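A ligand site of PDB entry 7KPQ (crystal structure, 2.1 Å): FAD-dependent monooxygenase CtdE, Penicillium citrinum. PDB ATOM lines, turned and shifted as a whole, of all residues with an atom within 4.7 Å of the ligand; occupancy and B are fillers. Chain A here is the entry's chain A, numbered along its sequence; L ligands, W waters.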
ATOM      1  N   VAL A  26     -28.614  23.763  -8.569  1.00  0.00           N
ATOM      2  CA  VAL A  26     -29.113  22.657  -9.378  1.00  0.00           C
ATOM      3  C   VAL A  26     -28.083  21.540  -9.387  1.00  0.00           C
ATOM      4  O   VAL A  26     -26.949  21.732  -9.866  1.00  0.00           O
ATOM      5  CB  VAL A  26     -29.459  23.113 -10.803  1.00  0.00           C
ATOM      6  CG1 VAL A  26     -29.989  21.933 -11.620  1.00  0.00           C
ATOM      7  CG2 VAL A  26     -30.490  24.232 -10.770  1.00  0.00           C
ATOM      8  N   GLY A  27     -28.477  20.372  -8.905  1.00  0.00           N
ATOM      9  CA  GLY A  27     -27.610  19.207  -8.905  1.00  0.00           C
ATOM     10  C   GLY A  27     -26.994  18.973  -7.534  1.00  0.00           C
ATOM     11  O   GLY A  27     -26.130  19.747  -7.098  1.00  0.00           O
ATOM     12  N   LEU A  28     -27.448  17.927  -6.842  1.00  0.00           N
ATOM     13  CA  LEU A  28     -26.984  17.617  -5.492  1.00  0.00           C
ATOM     14  C   LEU A  28     -25.976  16.474  -5.463  1.00  0.00           C
ATOM     15  O   LEU A  28     -26.200  15.435  -4.820  1.00  0.00           O
ATOM     16  CB  LEU A  28     -28.161  17.371  -4.560  1.00  0.00           C
ATOM     17  CG  LEU A  28     -28.902  18.691  -4.325  1.00  0.00           C
ATOM     18  CD1 LEU A  28     -29.851  18.553  -3.172  1.00  0.00           C
ATOM     19  CD2 LEU A  28     -27.893  19.808  -4.047  1.00  0.00           C
ATOM     20  N   GLY A  29     -24.870  16.650  -6.159  1.00  0.00           N
ATOM     21  CA  GLY A  29     -23.734  15.769  -6.013  1.00  0.00           C
ATOM     22  C   GLY A  29     -22.836  16.416  -4.973  1.00  0.00           C
ATOM     23  O   GLY A  29     -23.290  17.198  -4.136  1.00  0.00           O
ATOM     24  N   ILE A  30     -21.544  16.077  -5.015  1.00  0.00           N
ATOM     25  CA  ILE A  30     -20.604  16.662  -4.071  1.00  0.00           C
ATOM     26  C   ILE A  30     -20.599  18.189  -4.171  1.00  0.00           C
ATOM     27  O   ILE A  30     -20.655  18.892  -3.154  1.00  0.00           O
ATOM     28  CB  ILE A  30     -19.197  16.062  -4.230  1.00  0.00           C
ATOM     29  CG1 ILE A  30     -19.245  14.577  -3.881  1.00  0.00           C
ATOM     30  CG2 ILE A  30     -18.214  16.779  -3.339  1.00  0.00           C
ATOM     31  CD1 ILE A  30     -19.615  14.350  -2.412  1.00  0.00           C
ATOM     32  N   ALA A  31     -20.481  18.721  -5.388  1.00  0.00           N
ATOM     33  CA  ALA A  31     -20.383  20.169  -5.557  1.00  0.00           C
ATOM     34  C   ALA A  31     -21.641  20.861  -5.051  1.00  0.00           C
ATOM     35  O   ALA A  31     -21.557  21.845  -4.307  1.00  0.00           O
ATOM     36  CB  ALA A  31     -20.150  20.512  -7.031  1.00  0.00           C
ATOM     37  N   GLY A  32     -22.813  20.388  -5.451  1.00  0.00           N
ATOM     38  CA  GLY A  32     -24.043  21.064  -5.061  1.00  0.00           C
ATOM     39  C   GLY A  32     -24.307  20.979  -3.570  1.00  0.00           C
ATOM     40  O   GLY A  32     -24.821  21.916  -2.968  1.00  0.00           O
ATOM     41  N   PHE A  49     -32.106  21.708  -5.986  1.00  0.00           N
ATOM     42  CA  PHE A  49     -32.898  20.862  -6.857  1.00  0.00           C
ATOM     43  C   PHE A  49     -32.059  19.672  -7.302  1.00  0.00           C
ATOM     44  O   PHE A  49     -30.875  19.835  -7.630  1.00  0.00           O
ATOM     45  CB  PHE A  49     -33.415  21.652  -8.071  1.00  0.00           C
ATOM     46  CG  PHE A  49     -34.337  22.785  -7.703  1.00  0.00           C
ATOM     47  CD1 PHE A  49     -33.827  24.021  -7.329  1.00  0.00           C
ATOM     48  CD2 PHE A  49     -35.720  22.595  -7.684  1.00  0.00           C
ATOM     49  CE1 PHE A  49     -34.662  25.055  -6.983  1.00  0.00           C
ATOM     50  CE2 PHE A  49     -36.560  23.634  -7.330  1.00  0.00           C
ATOM     51  CZ  PHE A  49     -36.036  24.867  -6.984  1.00  0.00           C
ATOM     52  N   GLU A  50     -32.669  18.490  -7.315  1.00  0.00           N
ATOM     53  CA  GLU A  50     -31.995  17.271  -7.736  1.00  0.00           C
ATOM     54  C   GLU A  50     -32.948  16.505  -8.634  1.00  0.00           C
ATOM     55  O   GLU A  50     -34.140  16.400  -8.328  1.00  0.00           O
ATOM     56  CB  GLU A  50     -31.569  16.426  -6.513  1.00  0.00           C
ATOM     57  CG  GLU A  50     -31.163  14.987  -6.813  1.00  0.00           C
ATOM     58  CD  GLU A  50     -30.039  14.908  -7.859  1.00  0.00           C
ATOM     59  OE1 GLU A  50     -29.084  15.707  -7.766  1.00  0.00           O
ATOM     60  OE2 GLU A  50     -30.106  14.028  -8.750  1.00  0.00           O
ATOM     61  N   LYS A  51     -32.434  15.990  -9.762  1.00  0.00           N
ATOM     62  CA  LYS A  51     -33.307  15.329 -10.727  1.00  0.00           C
ATOM     63  C   LYS A  51     -33.772  13.949 -10.274  1.00  0.00           C
ATOM     64  O   LYS A  51     -34.912  13.562 -10.580  1.00  0.00           O
ATOM     65  CB  LYS A  51     -32.610  15.238 -12.095  1.00  0.00           C
ATOM     66  CG  LYS A  51     -31.745  14.005 -12.307  1.00  0.00           C
ATOM     67  CD  LYS A  51     -31.265  13.901 -13.744  1.00  0.00           C
ATOM     68  CE  LYS A  51     -29.997  13.037 -13.831  1.00  0.00           C
ATOM     69  NZ  LYS A  51     -29.568  12.805 -15.249  1.00  0.00           N
ATOM     70  N   THR A  52     -32.945  13.194  -9.550  1.00  0.00           N
ATOM     71  CA  THR A  52     -33.391  11.877  -9.130  1.00  0.00           C
ATOM     72  C   THR A  52     -34.544  12.001  -8.125  1.00  0.00           C
ATOM     73  O   THR A  52     -34.658  13.013  -7.419  1.00  0.00           O
ATOM     74  CB  THR A  52     -32.236  11.082  -8.510  1.00  0.00           C
ATOM     75  OG1 THR A  52     -31.743  11.764  -7.348  1.00  0.00           O
ATOM     76  CG2 THR A  52     -31.097  10.898  -9.519  1.00  0.00           C
ATOM     77  N   ILE A  58     -25.291   5.722  -5.248  1.00  0.00           N
ATOM     78  CA  ILE A  58     -24.569   5.102  -6.357  1.00  0.00           C
ATOM     79  C   ILE A  58     -23.176   5.710  -6.401  1.00  0.00           C
ATOM     80  O   ILE A  58     -22.984   6.885  -6.072  1.00  0.00           O
ATOM     81  CB  ILE A  58     -25.294   5.346  -7.699  1.00  0.00           C
ATOM     82  CG1 ILE A  58     -26.705   4.750  -7.673  1.00  0.00           C
ATOM     83  CG2 ILE A  58     -24.524   4.776  -8.867  1.00  0.00           C
ATOM     84  CD1 ILE A  58     -27.503   5.043  -8.920  1.00  0.00           C
ATOM     85  N   GLY A  59     -22.184   4.909  -6.790  1.00  0.00           N
ATOM     86  CA  GLY A  59     -20.881   5.516  -6.957  1.00  0.00           C
ATOM     87  C   GLY A  59     -19.695   4.585  -6.740  1.00  0.00           C
ATOM     88  O   GLY A  59     -19.815   3.503  -6.164  1.00  0.00           O
ATOM     89  N   ASP A  60     -18.539   5.058  -7.205  1.00  0.00           N
ATOM     90  CA  ASP A  60     -17.255   4.392  -7.073  1.00  0.00           C
ATOM     91  C   ASP A  60     -16.471   5.028  -5.958  1.00  0.00           C
ATOM     92  O   ASP A  60     -16.821   6.104  -5.450  1.00  0.00           O
ATOM     93  CB  ASP A  60     -16.460   4.486  -8.381  1.00  0.00           C
ATOM     94  CG  ASP A  60     -15.339   3.466  -8.471  1.00  0.00           C
ATOM     95  OD1 ASP A  60     -15.272   2.540  -7.621  1.00  0.00           O
ATOM     96  OD2 ASP A  60     -14.527   3.590  -9.408  1.00  0.00           O
ATOM     97  N   PHE A  62     -13.919   7.307  -4.538  1.00  0.00           N
ATOM     98  CA  PHE A  62     -13.121   8.450  -4.953  1.00  0.00           C
ATOM     99  C   PHE A  62     -12.291   8.864  -3.748  1.00  0.00           C
ATOM    100  O   PHE A  62     -12.343   8.225  -2.693  1.00  0.00           O
ATOM    101  CB  PHE A  62     -14.005   9.526  -5.644  1.00  0.00           C
ATOM    102  CG  PHE A  62     -15.066  10.179  -4.784  1.00  0.00           C
ATOM    103  CD1 PHE A  62     -15.203   9.927  -3.424  1.00  0.00           C
ATOM    104  CD2 PHE A  62     -15.987  11.016  -5.390  1.00  0.00           C
ATOM    105  CE1 PHE A  62     -16.212  10.555  -2.700  1.00  0.00           C
ATOM    106  CE2 PHE A  62     -17.001  11.637  -4.678  1.00  0.00           C
ATOM    107  CZ  PHE A  62     -17.115  11.404  -3.326  1.00  0.00           C
ATOM    108  N   ARG A 122     -18.166   6.883  -3.000  1.00  0.00           N
ATOM    109  CA  ARG A 122     -18.920   8.102  -3.290  1.00  0.00           C
ATOM    110  C   ARG A 122     -20.315   8.070  -2.661  1.00  0.00           C
ATOM    111  O   ARG A 122     -20.808   9.091  -2.178  1.00  0.00           O
ATOM    112  CB  ARG A 122     -19.023   8.310  -4.796  1.00  0.00           C
ATOM    113  CG  ARG A 122     -19.885   9.507  -5.159  1.00  0.00           C
ATOM    114  CD  ARG A 122     -20.392   9.469  -6.580  1.00  0.00           C
ATOM    115  NE  ARG A 122     -21.105  10.692  -6.886  1.00  0.00           N
ATOM    116  CZ  ARG A 122     -22.416  10.851  -6.713  1.00  0.00           C
ATOM    117  NH1 ARG A 122     -23.183   9.861  -6.290  1.00  0.00           N
ATOM    118  NH2 ARG A 122     -22.959  12.040  -6.969  1.00  0.00           N
ATOM    119  N   SER A 144     -36.587  16.794  -9.668  1.00  0.00           N
ATOM    120  CA  SER A 144     -36.588  18.119 -10.290  1.00  0.00           C
ATOM    121  C   SER A 144     -35.561  18.141 -11.412  1.00  0.00           C
ATOM    122  O   SER A 144     -34.394  18.497 -11.189  1.00  0.00           O
ATOM    123  CB  SER A 144     -36.292  19.207  -9.242  1.00  0.00           C
ATOM    124  OG  SER A 144     -37.220  19.146  -8.179  1.00  0.00           O
ATOM    125  N   ASN A 145     -35.978  17.769 -12.618  1.00  0.00           N
ATOM    126  CA  ASN A 145     -35.073  17.747 -13.770  1.00  0.00           C
ATOM    127  C   ASN A 145     -35.087  19.143 -14.386  1.00  0.00           C
ATOM    128  O   ASN A 145     -36.089  19.550 -14.980  1.00  0.00           O
ATOM    129  CB  ASN A 145     -35.488  16.685 -14.779  1.00  0.00           C
ATOM    130  CG  ASN A 145     -34.443  16.470 -15.859  1.00  0.00           C
ATOM    131  OD1 ASN A 145     -33.868  17.427 -16.389  1.00  0.00           O
ATOM    132  ND2 ASN A 145     -34.200  15.216 -16.204  1.00  0.00           N
ATOM    133  N   VAL A 146     -33.971  19.860 -14.288  1.00  0.00           N
ATOM    134  CA  VAL A 146     -33.887  21.246 -14.719  1.00  0.00           C
ATOM    135  C   VAL A 146     -33.152  21.304 -16.047  1.00  0.00           C
ATOM    136  O   VAL A 146     -32.044  20.788 -16.170  1.00  0.00           O
ATOM    137  CB  VAL A 146     -33.170  22.110 -13.660  1.00  0.00           C
ATOM    138  CG1 VAL A 146     -33.200  23.578 -14.077  1.00  0.00           C
ATOM    139  CG2 VAL A 146     -33.798  21.899 -12.289  1.00  0.00           C
ATOM    140  N   THR A 173     -24.535  22.732 -10.641  1.00  0.00           N
ATOM    141  CA  THR A 173     -23.583  21.688 -10.298  1.00  0.00           C
ATOM    142  C   THR A 173     -24.174  20.342 -10.720  1.00  0.00           C
ATOM    143  O   THR A 173     -24.224  19.384  -9.941  1.00  0.00           O
ATOM    144  CB  THR A 173     -23.250  21.740  -8.815  1.00  0.00           C
ATOM    145  OG1 THR A 173     -24.452  21.854  -8.057  1.00  0.00           O
ATOM    146  CG2 THR A 173     -22.341  22.939  -8.501  1.00  0.00           C
ATOM    147  N   ASP A 174     -24.617  20.258 -11.959  1.00  0.00           N
ATOM    148  CA  ASP A 174     -25.339  19.099 -12.445  1.00  0.00           C
ATOM    149  C   ASP A 174     -24.452  18.056 -13.128  1.00  0.00           C
ATOM    150  O   ASP A 174     -24.969  17.186 -13.835  1.00  0.00           O
ATOM    151  CB  ASP A 174     -26.521  19.537 -13.327  1.00  0.00           C
ATOM    152  CG  ASP A 174     -26.132  20.381 -14.515  1.00  0.00           C
ATOM    153  OD1 ASP A 174     -25.068  21.046 -14.490  1.00  0.00           O
ATOM    154  OD2 ASP A 174     -26.947  20.438 -15.459  1.00  0.00           O
ATOM    155  N   GLY A 175     -23.123  18.170 -12.988  1.00  0.00           N
ATOM    156  CA  GLY A 175     -22.234  17.094 -13.395  1.00  0.00           C
ATOM    157  C   GLY A 175     -21.795  17.141 -14.844  1.00  0.00           C
ATOM    158  O   GLY A 175     -22.153  18.028 -15.616  1.00  0.00           O
ATOM    159  N   LYS A 179     -26.807  19.801 -18.345  1.00  0.00           N
ATOM    160  CA  LYS A 179     -27.716  20.512 -19.228  1.00  0.00           C
ATOM    161  C   LYS A 179     -27.576  22.008 -18.993  1.00  0.00           C
ATOM    162  O   LYS A 179     -27.830  22.805 -19.899  1.00  0.00           O
ATOM    163  CB  LYS A 179     -29.163  20.082 -18.973  1.00  0.00           C
ATOM    164  CG  LYS A 179     -29.493  18.669 -19.438  1.00  0.00           C
ATOM    165  CD  LYS A 179     -29.136  18.462 -20.889  1.00  0.00           C
ATOM    166  CE  LYS A 179     -29.503  17.050 -21.326  1.00  0.00           C
ATOM    167  NZ  LYS A 179     -28.543  16.044 -20.765  1.00  0.00           N
ATOM    168  N   ARG A 200     -17.639  -1.400 -13.643  1.00  0.00           N
ATOM    169  CA  ARG A 200     -17.418  -1.392 -12.210  1.00  0.00           C
ATOM    170  C   ARG A 200     -18.695  -1.722 -11.468  1.00  0.00           C
ATOM    171  O   ARG A 200     -19.807  -1.581 -11.999  1.00  0.00           O
ATOM    172  CB  ARG A 200     -16.883  -0.038 -11.725  1.00  0.00           C
ATOM    173  CG  ARG A 200     -17.780   1.133 -12.071  1.00  0.00           C
ATOM    174  CD  ARG A 200     -17.448   2.277 -11.157  1.00  0.00           C
ATOM    175  NE  ARG A 200     -17.264   1.785  -9.804  1.00  0.00           N
ATOM    176  CZ  ARG A 200     -18.231   1.641  -8.892  1.00  0.00           C
ATOM    177  NH1 ARG A 200     -19.470   2.016  -9.146  1.00  0.00           N
ATOM    178  NH2 ARG A 200     -17.920   1.138  -7.698  1.00  0.00           N
ATOM    179  N   TRP A 264     -23.674   7.938 -16.010  1.00  0.00           N
ATOM    180  CA  TRP A 264     -23.112   7.190 -14.891  1.00  0.00           C
ATOM    181  C   TRP A 264     -23.899   5.925 -14.536  1.00  0.00           C
ATOM    182  O   TRP A 264     -23.374   5.100 -13.790  1.00  0.00           O
ATOM    183  CB  TRP A 264     -23.003   8.091 -13.649  1.00  0.00           C
ATOM    184  CG  TRP A 264     -21.985   9.193 -13.758  1.00  0.00           C
ATOM    185  CD1 TRP A 264     -22.217  10.536 -13.776  1.00  0.00           C
ATOM    186  CD2 TRP A 264     -20.551   9.038 -13.829  1.00  0.00           C
ATOM    187  NE1 TRP A 264     -21.034  11.224 -13.867  1.00  0.00           N
ATOM    188  CE2 TRP A 264     -19.999  10.328 -13.908  1.00  0.00           C
ATOM    189  CE3 TRP A 264     -19.691   7.930 -13.849  1.00  0.00           C
ATOM    190  CZ2 TRP A 264     -18.624  10.547 -13.999  1.00  0.00           C
ATOM    191  CZ3 TRP A 264     -18.325   8.146 -13.944  1.00  0.00           C
ATOM    192  CH2 TRP A 264     -17.805   9.451 -14.013  1.00  0.00           C
ATOM    193  N   ILE A 265     -25.112   5.737 -15.056  1.00  0.00           N
ATOM    194  CA  ILE A 265     -25.918   4.592 -14.644  1.00  0.00           C
ATOM    195  C   ILE A 265     -26.160   3.617 -15.780  1.00  0.00           C
ATOM    196  O   ILE A 265     -26.998   2.718 -15.670  1.00  0.00           O
ATOM    197  CB  ILE A 265     -27.245   5.026 -14.000  1.00  0.00           C
ATOM    198  CG1 ILE A 265     -28.109   5.813 -14.997  1.00  0.00           C
ATOM    199  CG2 ILE A 265     -26.997   5.828 -12.720  1.00  0.00           C
ATOM    200  CD1 ILE A 265     -29.478   6.185 -14.465  1.00  0.00           C
ATOM    201  N   HIS A 301     -18.980   2.811 -17.932  1.00  0.00           N
ATOM    202  CA  HIS A 301     -18.685   4.232 -18.063  1.00  0.00           C
ATOM    203  C   HIS A 301     -17.561   4.486 -19.058  1.00  0.00           C
ATOM    204  O   HIS A 301     -16.616   3.706 -19.152  1.00  0.00           O
ATOM    205  CB  HIS A 301     -18.206   4.895 -16.744  1.00  0.00           C
ATOM    206  CG  HIS A 301     -19.082   4.653 -15.556  1.00  0.00           C
ATOM    207  ND1 HIS A 301     -18.554   4.381 -14.312  1.00  0.00           N
ATOM    208  CD2 HIS A 301     -20.425   4.694 -15.408  1.00  0.00           C
ATOM    209  CE1 HIS A 301     -19.546   4.244 -13.447  1.00  0.00           C
ATOM    210  NE2 HIS A 301     -20.689   4.428 -14.085  1.00  0.00           N
ATOM    211  N   LEU A 322     -20.322  24.901 -11.911  1.00  0.00           N
ATOM    212  CA  LEU A 322     -19.194  24.492 -11.078  1.00  0.00           C
ATOM    213  C   LEU A 322     -19.129  22.965 -11.049  1.00  0.00           C
ATOM    214  O   LEU A 322     -20.005  22.281 -11.590  1.00  0.00           O
ATOM    215  CB  LEU A 322     -19.323  25.091  -9.679  1.00  0.00           C
ATOM    216  CG  LEU A 322     -19.329  26.625  -9.596  1.00  0.00           C
ATOM    217  CD1 LEU A 322     -19.755  27.106  -8.200  1.00  0.00           C
ATOM    218  CD2 LEU A 322     -17.963  27.211  -9.996  1.00  0.00           C
ATOM    219  N   GLY A 323     -18.099  22.436 -10.387  1.00  0.00           N
ATOM    220  CA  GLY A 323     -17.924  20.995 -10.356  1.00  0.00           C
ATOM    221  C   GLY A 323     -17.608  20.403 -11.715  1.00  0.00           C
ATOM    222  O   GLY A 323     -17.028  21.045 -12.599  1.00  0.00           O
ATOM    223  N   ASP A 324     -18.011  19.133 -11.886  1.00  0.00           N
ATOM    224  CA  ASP A 324     -17.782  18.442 -13.147  1.00  0.00           C
ATOM    225  C   ASP A 324     -18.519  19.079 -14.310  1.00  0.00           C
ATOM    226  O   ASP A 324     -18.131  18.871 -15.468  1.00  0.00           O
ATOM    227  CB  ASP A 324     -18.226  16.980 -13.040  1.00  0.00           C
ATOM    228  CG  ASP A 324     -17.166  16.087 -12.445  1.00  0.00           C
ATOM    229  OD1 ASP A 324     -16.201  16.605 -11.840  1.00  0.00           O
ATOM    230  OD2 ASP A 324     -17.303  14.854 -12.592  1.00  0.00           O
ATOM    231  N   ALA A 325     -19.601  19.817 -14.050  1.00  0.00           N
ATOM    232  CA  ALA A 325     -20.276  20.543 -15.114  1.00  0.00           C
ATOM    233  C   ALA A 325     -19.325  21.529 -15.791  1.00  0.00           C
ATOM    234  O   ALA A 325     -19.416  21.751 -16.998  1.00  0.00           O
ATOM    235  CB  ALA A 325     -21.511  21.273 -14.561  1.00  0.00           C
ATOM    236  N   GLY A 336     -11.681  15.164  -8.693  1.00  0.00           N
ATOM    237  CA  GLY A 336     -13.060  15.515  -8.999  1.00  0.00           C
ATOM    238  C   GLY A 336     -13.847  15.970  -7.771  1.00  0.00           C
ATOM    239  O   GLY A 336     -14.444  17.045  -7.771  1.00  0.00           O
ATOM    240  N   ALA A 337     -13.861  15.145  -6.726  1.00  0.00           N
ATOM    241  CA  ALA A 337     -14.578  15.506  -5.508  1.00  0.00           C
ATOM    242  C   ALA A 337     -13.923  16.696  -4.811  1.00  0.00           C
ATOM    243  O   ALA A 337     -14.615  17.597  -4.344  1.00  0.00           O
ATOM    244  CB  ALA A 337     -14.645  14.305  -4.566  1.00  0.00           C
ATOM    245  N   ALA A 340     -14.778  19.917  -6.587  1.00  0.00           N
ATOM    246  CA  ALA A 340     -16.189  20.194  -6.331  1.00  0.00           C
ATOM    247  C   ALA A 340     -16.374  20.841  -4.967  1.00  0.00           C
ATOM    248  O   ALA A 340     -17.152  21.790  -4.826  1.00  0.00           O
ATOM    249  CB  ALA A 340     -17.001  18.900  -6.430  1.00  0.00           C
HETATM  250  P1  LIG L   1     -21.929  14.863  -9.772  1.00  0.00           P
HETATM  251  O1  LIG L   1     -21.959  14.079 -11.037  1.00  0.00           O
HETATM  252  O2  LIG L   1     -21.339  14.125  -8.576  1.00  0.00           O
HETATM  253  O3  LIG L   1     -23.384  15.310  -9.347  1.00  0.00           O
HETATM  254  C1  LIG L   1     -24.255  16.010 -10.252  1.00  0.00           C
HETATM  255  C2  LIG L   1     -25.660  15.894  -9.715  1.00  0.00           C
HETATM  256  O4  LIG L   1     -26.577  16.649 -10.536  1.00  0.00           O
HETATM  257  C3  LIG L   1     -26.212  14.465  -9.642  1.00  0.00           C
HETATM  258  O5  LIG L   1     -26.809  14.235  -8.370  1.00  0.00           O
HETATM  259  C4  LIG L   1     -27.254  14.432 -10.777  1.00  0.00           C
HETATM  260  O6  LIG L   1     -28.319  13.538 -10.466  1.00  0.00           O
HETATM  261  C5  LIG L   1     -27.736  15.877 -10.774  1.00  0.00           C
HETATM  262  N1  LIG L   1     -28.313  16.315 -12.043  1.00  0.00           N
HETATM  263  C6  LIG L   1     -27.856  16.044 -13.305  1.00  0.00           C
HETATM  264  N2  LIG L   1     -28.554  16.600 -14.260  1.00  0.00           N
HETATM  265  C7  LIG L   1     -29.541  17.305 -13.585  1.00  0.00           C
HETATM  266  C8  LIG L   1     -30.608  18.105 -14.034  1.00  0.00           C
HETATM  267  N3  LIG L   1     -30.863  18.346 -15.318  1.00  0.00           N
HETATM  268  N4  LIG L   1     -31.406  18.669 -13.088  1.00  0.00           N
HETATM  269  C9  LIG L   1     -31.142  18.431 -11.800  1.00  0.00           C
HETATM  270  N5  LIG L   1     -30.179  17.683 -11.264  1.00  0.00           N
HETATM  271  C10 LIG L   1     -29.401  17.143 -12.208  1.00  0.00           C
HETATM  272  N6  LIG L   1     -17.087   9.702 -10.843  1.00  0.00           N
HETATM  273  C11 LIG L   1     -16.108   8.765 -10.977  1.00  0.00           C
HETATM  274  O7  LIG L   1     -14.917   9.069 -11.126  1.00  0.00           O
HETATM  275  N7  LIG L   1     -16.445   7.413 -10.947  1.00  0.00           N
HETATM  276  C12 LIG L   1     -17.722   6.901 -10.799  1.00  0.00           C
HETATM  277  O8  LIG L   1     -17.905   5.681 -10.789  1.00  0.00           O
HETATM  278  C13 LIG L   1     -18.755   7.912 -10.647  1.00  0.00           C
HETATM  279  N8  LIG L   1     -19.985   7.505 -10.496  1.00  0.00           N
HETATM  280  C14 LIG L   1     -20.970   8.472 -10.368  1.00  0.00           C
HETATM  281  C15 LIG L   1     -22.294   8.055 -10.208  1.00  0.00           C
HETATM  282  C16 LIG L   1     -23.326   8.986 -10.079  1.00  0.00           C
HETATM  283  C17 LIG L   1     -24.735   8.499  -9.913  1.00  0.00           C
HETATM  284  C18 LIG L   1     -23.022  10.362 -10.104  1.00  0.00           C
HETATM  285  C19 LIG L   1     -24.115  11.389  -9.960  1.00  0.00           C
HETATM  286  C20 LIG L   1     -21.703  10.774 -10.252  1.00  0.00           C
HETATM  287  C21 LIG L   1     -20.680   9.840 -10.385  1.00  0.00           C
HETATM  288  N9  LIG L   1     -19.333  10.233 -10.530  1.00  0.00           N
HETATM  289  C22 LIG L   1     -18.339   9.285 -10.688  1.00  0.00           C
HETATM  290  C23 LIG L   1     -18.963  11.655 -10.601  1.00  0.00           C
HETATM  291  C24 LIG L   1     -18.277  12.193  -9.344  1.00  0.00           C
HETATM  292  O9  LIG L   1     -19.207  12.308  -8.269  1.00  0.00           O
HETATM  293  C25 LIG L   1     -17.690  13.570  -9.665  1.00  0.00           C
HETATM  294  O10 LIG L   1     -16.570  13.397 -10.524  1.00  0.00           O
HETATM  295  C26 LIG L   1     -17.268  14.426  -8.469  1.00  0.00           C
HETATM  296  O11 LIG L   1     -16.807  13.600  -7.402  1.00  0.00           O
HETATM  297  C27 LIG L   1     -18.361  15.363  -8.007  1.00  0.00           C
HETATM  298  O12 LIG L   1     -18.775  16.188  -9.122  1.00  0.00           O
HETATM  299  P2  LIG L   1     -20.112  17.020  -9.087  1.00  0.00           P
HETATM  300  O13 LIG L   1     -19.841  18.355  -9.798  1.00  0.00           O
HETATM  301  O14 LIG L   1     -20.646  17.160  -7.704  1.00  0.00           O
HETATM  302  O15 LIG L   1     -21.152  16.220  -9.999  1.00  0.00           O
HETATM  303  O   HOH W   1     -16.978   8.093  -8.181  1.00  0.00           O
HETATM  304  O   HOH W   2     -27.770  10.904 -11.037  1.00  0.00           O
HETATM  305  O   HOH W   3     -29.488  21.420 -15.488  1.00  0.00           O
HETATM  306  O   HOH W   4     -14.725  11.323 -12.446  1.00  0.00           O
HETATM  307  O   HOH W   5     -25.807  12.734  -6.494  1.00  0.00           O
HETATM  308  O   HOH W   6     -29.754  15.446 -17.126  1.00  0.00           O
HETATM  309  O   HOH W   7     -14.991   4.707 -12.023  1.00  0.00           O
HETATM  310  O   HOH W   8     -12.708   7.671 -10.154  1.00  0.00           O
HETATM  311  O   HOH W   9     -31.893  16.589 -17.820  1.00  0.00           O
HETATM  312  O   HOH W  10     -21.229  19.783 -11.524  1.00  0.00           O
HETATM  313  O   HOH W  11     -23.198  18.429  -7.538  1.00  0.00           O
HETATM  314  O   HOH W  12     -27.785  18.010 -16.796  1.00  0.00           O
HETATM  315  O   HOH W  13     -23.728  13.576 -12.984  1.00  0.00           O
HETATM  316  O   HOH W  14     -20.212  14.149 -13.167  1.00  0.00           O
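OE2 of Glu 50 sits at hydrogen-bond distance from N of Thr 52 (3.1 Å).
N of Thr 173 sits at hydrogen-bond distance from O of Val 26 (2.7 Å).
The backbone carbonyl oxygen (O) of Trp 264 lies within hydrogen-bond range of a ring nitrogen (NE2) of His 301, at 2.8 Å.
The guanidinium group (NH1) of Arg 122 sits at hydrogen-bond distance from the backbone carbonyl oxygen (O) of Ile 58 (3.0 Å).
N of Asp 174 sits at hydrogen-bond distance from O of Val 26, at 3.5 Å.
The backbone carbonyl oxygen of Gly 175 lies close to the backbone NH of Ala 325, 3.5 Å away.
N of Arg 122 sits at hydrogen-bond distance from O of Asp 60 (2.9 Å).
The backbone NH (N) of Gly 27 lies within hydrogen-bond range of the backbone carbonyl oxygen (O) of Phe 49 (2.8 Å).
Water W5 lies within hydrogen-bond range of O5 of the ligand, NH2 of Arg 122 and O of Leu 28.
Water W14 lies within hydrogen-bond range of an oxygen (O1) of the ligand (2.8 Å), the side-chain carboxylate of Asp 324 (3.0 Å) and the indole nitrogen of Trp 264 (3.1 Å).
Water W12 lies within hydrogen-bond range of N of Lys 179, OD2 of Asp 174 and N2 of the ligand.
Water W9 bridges OD1 of Asn 145 (2.6 Å) and N3 of the ligand (3.2 Å).
Water W7 bridges the side-chain carboxylate of Asp 60 (2.9 Å) and a nitrogen (N7) of the ligand (3.3 Å).
Water W6 lies within hydrogen-bond range of the side-chain amino group (NZ) of Lys 51 (3.2 Å) and a nitrogen (N2) of the ligand (3.3 Å).
Merely in contact with the ligand: Asp 60 (3.1 Å), Asp 174 (3.1 Å), Gly 27 (3.2 Å), Trp 264 (3.3 Å), Ser 144 (3.3 Å), Gly 323 (3.3 Å), Phe 62 (3.4 Å), Gly 29 (3.4 Å), Thr 173 (3.4 Å), His 301 (3.4 Å), Arg 200 (3.5 Å), Gly 175 (3.7 Å), Val 26 (3.7 Å), Leu 28 (3.8 Å), Gly 336 (3.8 Å), Ile 58 (3.9 Å) and Thr 52 (3.9 Å).
Hydrophobic or aromatic side chains that line the ligand: Val 26, Ile 30, Ala 31, Ile 58, Phe 62, Val 146, Trp 264, His 301 and Ala 337.
Along chain A the residues within 4 Å of the ligand span positions 26 to 337.
The nearest printed residue that does not touch the ligand is Ala 340 (4.1 Å).
O14 of the ligand lies within hydrogen-bond range of N of Ile 30 (3.0 Å).
An oxygen (O10) of the ligand sits at hydrogen-bond distance from the side-chain carboxylate of Asp 324, 2.6 Å away.
NH2 of Arg 122 lies within salt-bridge range of O2 of the ligand (3.1 Å).
A nitrogen (N4) of the ligand lies within hydrogen-bond range of the backbone NH (N) of Val 146 (3.1 Å).
OD1 of Asn 145 sits at hydrogen-bond distance from N3 of the ligand, 3.3 Å away.
N of Ala 31 lies within hydrogen-bond range of O14 of the ligand, at 2.8 Å.
The side-chain carboxylate of Glu 50 lies within hydrogen-bond range of an oxygen (O6) of the ligand (2.5 Å).
The backbone NH (N) of Lys 51 sits at hydrogen-bond distance from a nitrogen (N5) of the ligand, at 3.2 Å.
The backbone NH of Asp 324 sits at hydrogen-bond distance from an oxygen (O13) of the ligand, at 2.9 Å.
O of Val 146 is in hydrogen-bond range of N3 of the ligand (2.8 Å).
O11 of the ligand sits at hydrogen-bond distance from N of Ala 337.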
